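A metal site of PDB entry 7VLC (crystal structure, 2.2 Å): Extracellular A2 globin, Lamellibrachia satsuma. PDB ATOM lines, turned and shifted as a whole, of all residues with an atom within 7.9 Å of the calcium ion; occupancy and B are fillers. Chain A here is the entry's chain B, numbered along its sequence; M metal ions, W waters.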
ATOM      1  N   ALA A 102       2.196 -12.197 -29.802  1.00  0.00           N
ATOM      2  CA  ALA A 102       2.365 -11.499 -28.529  1.00  0.00           C
ATOM      3  C   ALA A 102       1.871 -12.345 -27.359  1.00  0.00           C
ATOM      4  O   ALA A 102       2.309 -12.146 -26.226  1.00  0.00           O
ATOM      5  CB  ALA A 102       1.640 -10.159 -28.556  1.00  0.00           C
ATOM      6  N   GLU A 103       0.934 -13.265 -27.617  1.00  0.00           N
ATOM      7  CA  GLU A 103       0.486 -14.183 -26.573  1.00  0.00           C
ATOM      8  C   GLU A 103       1.610 -15.123 -26.141  1.00  0.00           C
ATOM      9  O   GLU A 103       1.766 -15.413 -24.955  1.00  0.00           O
ATOM     10  CB  GLU A 103      -0.717 -14.987 -27.065  1.00  0.00           C
ATOM     11  CG  GLU A 103      -1.500 -15.679 -25.964  1.00  0.00           C
ATOM     12  CD  GLU A 103      -2.307 -14.705 -25.133  1.00  0.00           C
ATOM     13  OE1 GLU A 103      -3.092 -13.918 -25.720  1.00  0.00           O
ATOM     14  OE2 GLU A 103      -2.156 -14.706 -23.886  1.00  0.00           O
ATOM     15  N   TYR A 105       5.011 -14.674 -26.418  1.00  0.00           N
ATOM     16  CA  TYR A 105       6.052 -13.971 -25.677  1.00  0.00           C
ATOM     17  C   TYR A 105       5.677 -13.829 -24.211  1.00  0.00           C
ATOM     18  O   TYR A 105       6.559 -13.883 -23.343  1.00  0.00           O
ATOM     19  CB  TYR A 105       6.309 -12.592 -26.299  1.00  0.00           C
ATOM     20  CG  TYR A 105       7.260 -12.596 -27.480  1.00  0.00           C
ATOM     21  CD1 TYR A 105       8.625 -12.778 -27.291  1.00  0.00           C
ATOM     22  CD2 TYR A 105       6.799 -12.401 -28.772  1.00  0.00           C
ATOM     23  CE1 TYR A 105       9.500 -12.775 -28.360  1.00  0.00           C
ATOM     24  CE2 TYR A 105       7.670 -12.403 -29.854  1.00  0.00           C
ATOM     25  CZ  TYR A 105       9.014 -12.597 -29.642  1.00  0.00           C
ATOM     26  OH  TYR A 105       9.891 -12.601 -30.701  1.00  0.00           O
ATOM     27  N   ASN A 106       4.382 -13.660 -23.911  1.00  0.00           N
ATOM     28  CA  ASN A 106       3.956 -13.599 -22.518  1.00  0.00           C
ATOM     29  C   ASN A 106       3.968 -14.967 -21.868  1.00  0.00           C
ATOM     30  O   ASN A 106       4.184 -15.075 -20.654  1.00  0.00           O
ATOM     31  CB  ASN A 106       2.567 -12.968 -22.414  1.00  0.00           C
ATOM     32  CG  ASN A 106       2.576 -11.484 -22.686  1.00  0.00           C
ATOM     33  OD1 ASN A 106       3.610 -10.821 -22.575  1.00  0.00           O
ATOM     34  ND2 ASN A 106       1.416 -10.944 -23.049  1.00  0.00           N
ATOM     35  N   VAL A 107       3.732 -16.032 -22.641  1.00  0.00           N
ATOM     36  CA  VAL A 107       3.788 -17.379 -22.087  1.00  0.00           C
ATOM     37  C   VAL A 107       5.209 -17.705 -21.624  1.00  0.00           C
ATOM     38  O   VAL A 107       5.434 -18.132 -20.499  1.00  0.00           O
ATOM     39  CB  VAL A 107       3.284 -18.414 -23.119  1.00  0.00           C
ATOM     40  CG1 VAL A 107       3.650 -19.827 -22.674  1.00  0.00           C
ATOM     41  CG2 VAL A 107       1.778 -18.279 -23.294  1.00  0.00           C
ATOM     42  N   GLU A 109       7.441 -15.497 -21.066  1.00  0.00           N
ATOM     43  CA  GLU A 109       7.631 -14.537 -19.979  1.00  0.00           C
ATOM     44  C   GLU A 109       7.225 -15.154 -18.639  1.00  0.00           C
ATOM     45  O   GLU A 109       7.973 -15.087 -17.651  1.00  0.00           O
ATOM     46  CB  GLU A 109       6.816 -13.287 -20.261  1.00  0.00           C
ATOM     47  CG  GLU A 109       7.540 -11.968 -20.121  1.00  0.00           C
ATOM     48  CD  GLU A 109       6.658 -10.787 -20.519  1.00  0.00           C
ATOM     49  OE1 GLU A 109       6.242 -10.012 -19.632  1.00  0.00           O
ATOM     50  OE2 GLU A 109       6.364 -10.646 -21.726  1.00  0.00           O
ATOM     51  N   HIS A 110       6.040 -15.765 -18.596  1.00  0.00           N
ATOM     52  CA  HIS A 110       5.555 -16.347 -17.342  1.00  0.00           C
ATOM     53  C   HIS A 110       6.372 -17.557 -16.937  1.00  0.00           C
ATOM     54  O   HIS A 110       6.618 -17.780 -15.745  1.00  0.00           O
ATOM     55  CB  HIS A 110       4.073 -16.704 -17.487  1.00  0.00           C
ATOM     56  CG  HIS A 110       3.453 -17.191 -16.217  1.00  0.00           C
ATOM     57  ND1 HIS A 110       3.145 -18.512 -15.996  1.00  0.00           N
ATOM     58  CD2 HIS A 110       3.087 -16.528 -15.085  1.00  0.00           C
ATOM     59  CE1 HIS A 110       2.616 -18.655 -14.797  1.00  0.00           C
ATOM     60  NE2 HIS A 110       2.573 -17.463 -14.225  1.00  0.00           N
ATOM     61  N   MET A 113       9.557 -16.351 -15.402  1.00  0.00           N
ATOM     62  CA  MET A 113       9.297 -15.862 -14.052  1.00  0.00           C
ATOM     63  C   MET A 113       9.059 -17.015 -13.080  1.00  0.00           C
ATOM     64  O   MET A 113       9.567 -16.991 -11.956  1.00  0.00           O
ATOM     65  CB  MET A 113       8.092 -14.915 -14.061  1.00  0.00           C
ATOM     66  CG  MET A 113       8.330 -13.650 -14.871  1.00  0.00           C
ATOM     67  SD  MET A 113       6.896 -12.556 -14.926  1.00  0.00           S
ATOM     68  CE  MET A 113       6.804 -12.034 -13.225  1.00  0.00           C
ATOM     69  N   GLN A 131       8.253  -8.551 -13.930  1.00  0.00           N
ATOM     70  CA  GLN A 131       7.252  -8.364 -14.965  1.00  0.00           C
ATOM     71  C   GLN A 131       7.525  -7.114 -15.790  1.00  0.00           C
ATOM     72  O   GLN A 131       7.410  -7.137 -17.024  1.00  0.00           O
ATOM     73  CB  GLN A 131       5.857  -8.296 -14.348  1.00  0.00           C
ATOM     74  CG  GLN A 131       4.718  -8.289 -15.365  1.00  0.00           C
ATOM     75  CD  GLN A 131       4.609  -9.601 -16.127  1.00  0.00           C
ATOM     76  OE1 GLN A 131       4.011 -10.565 -15.654  1.00  0.00           O
ATOM     77  NE2 GLN A 131       5.193  -9.637 -17.319  1.00  0.00           N
ATOM     78  N   ALA A 132       7.927  -6.032 -15.135  1.00  0.00           N
ATOM     79  CA  ALA A 132       8.128  -4.769 -15.836  1.00  0.00           C
ATOM     80  C   ALA A 132       9.369  -4.810 -16.723  1.00  0.00           C
ATOM     81  O   ALA A 132       9.375  -4.225 -17.809  1.00  0.00           O
ATOM     82  CB  ALA A 132       8.212  -3.617 -14.834  1.00  0.00           C
ATOM     83  N   LEU A 134      10.953  -7.682 -17.935  1.00  0.00           N
ATOM     84  CA  LEU A 134      10.788  -8.625 -19.031  1.00  0.00           C
ATOM     85  C   LEU A 134       9.889  -8.061 -20.126  1.00  0.00           C
ATOM     86  O   LEU A 134      10.069  -8.376 -21.310  1.00  0.00           O
ATOM     87  CB  LEU A 134      10.218  -9.952 -18.526  1.00  0.00           C
ATOM     88  CG  LEU A 134      11.214 -10.870 -17.818  1.00  0.00           C
ATOM     89  CD1 LEU A 134      10.520 -12.112 -17.278  1.00  0.00           C
ATOM     90  CD2 LEU A 134      12.340 -11.246 -18.761  1.00  0.00           C
ATOM     91  N   ASP A 135       8.909  -7.225 -19.752  1.00  0.00           N
ATOM     92  CA  ASP A 135       8.119  -6.506 -20.757  1.00  0.00           C
ATOM     93  C   ASP A 135       9.028  -5.666 -21.647  1.00  0.00           C
ATOM     94  O   ASP A 135       8.904  -5.687 -22.869  1.00  0.00           O
ATOM     95  CB  ASP A 135       7.074  -5.620 -20.080  1.00  0.00           C
ATOM     96  CG  ASP A 135       5.858  -6.408 -19.618  1.00  0.00           C
ATOM     97  OD1 ASP A 135       5.600  -7.496 -20.161  1.00  0.00           O
ATOM     98  OD2 ASP A 135       5.153  -5.924 -18.706  1.00  0.00           O
ATOM     99  N   VAL A 136       9.966  -4.944 -21.033  1.00  0.00           N
ATOM    100  CA  VAL A 136      10.920  -4.133 -21.793  1.00  0.00           C
ATOM    101  C   VAL A 136      11.721  -5.015 -22.751  1.00  0.00           C
ATOM    102  O   VAL A 136      12.028  -4.598 -23.884  1.00  0.00           O
ATOM    103  CB  VAL A 136      11.840  -3.350 -20.832  1.00  0.00           C
ATOM    104  CG1 VAL A 136      12.910  -2.600 -21.610  1.00  0.00           C
ATOM    105  CG2 VAL A 136      11.028  -2.390 -19.985  1.00  0.00           C
ATOM    106  N   THR A 138      10.893  -8.284 -23.996  1.00  0.00           N
ATOM    107  CA  THR A 138      10.061  -8.904 -25.030  1.00  0.00           C
ATOM    108  C   THR A 138       9.549  -7.864 -26.020  1.00  0.00           C
ATOM    109  O   THR A 138       9.519  -8.116 -27.234  1.00  0.00           O
ATOM    110  CB  THR A 138       8.890  -9.655 -24.403  1.00  0.00           C
ATOM    111  OG1 THR A 138       8.055  -8.738 -23.685  1.00  0.00           O
ATOM    112  CG2 THR A 138       9.389 -10.742 -23.461  1.00  0.00           C
ATOM    113  N   SER A 139       9.160  -6.686 -25.526  1.00  0.00           N
ATOM    114  CA  SER A 139       8.675  -5.633 -26.416  1.00  0.00           C
ATOM    115  C   SER A 139       9.742  -5.189 -27.412  1.00  0.00           C
ATOM    116  O   SER A 139       9.418  -4.775 -28.531  1.00  0.00           O
ATOM    117  CB  SER A 139       8.173  -4.445 -25.605  1.00  0.00           C
ATOM    118  OG  SER A 139       7.635  -3.446 -26.447  1.00  0.00           O
ATOM    119  N   GLN A 142       9.959  -7.936 -30.260  1.00  0.00           N
ATOM    120  CA  GLN A 142       8.852  -7.858 -31.198  1.00  0.00           C
ATOM    121  C   GLN A 142       8.909  -6.615 -32.083  1.00  0.00           C
ATOM    122  O   GLN A 142       7.898  -6.248 -32.682  1.00  0.00           O
ATOM    123  CB  GLN A 142       7.510  -7.892 -30.452  1.00  0.00           C
ATOM    124  CG  GLN A 142       7.376  -9.026 -29.455  1.00  0.00           C
ATOM    125  CD  GLN A 142       6.002  -9.079 -28.821  1.00  0.00           C
ATOM    126  OE1 GLN A 142       5.007  -9.345 -29.485  1.00  0.00           O
ATOM    127  NE2 GLN A 142       5.947  -8.831 -27.520  1.00  0.00           N
HETATM  128 CA    CA M   1       4.448  -9.130 -21.256  1.00  0.00          CA
HETATM  129  O   HOH W   1       5.373  -8.374 -23.286  1.00  0.00           O
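The side-chain amide nitrogen (NE2) of Gln 131 sits close to the side-chain carboxylate (OE1) of Glu 109 (2.6 Å). The backbone carbonyl oxygen (O) of Asp 135 sits at hydrogen-bond distance from the side-chain hydroxyl (OG1) of Thr 138 (3.3 Å). The side-chain hydroxyl of Thr 138 sits close to the side-chain carboxylate of Glu 109.
Of the 16 residues printed, 3 come within 4 Å of the calcium ion. Along chain A the residues within 4 Å of the calcium ion span positions 106 to 135.
The calcium ion is bound by the side-chain carboxylate (OD1) of Asp 135 (2.3 Å), the side-chain amide oxygen (OD1) of Asn 106 (2.3 Å), water W1 (2.4 Å), the side-chain carboxylate (OE2) of Glu 109 (2.5 Å) and the side-chain carboxylate (OE1) of Glu 109 (2.6 Å).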
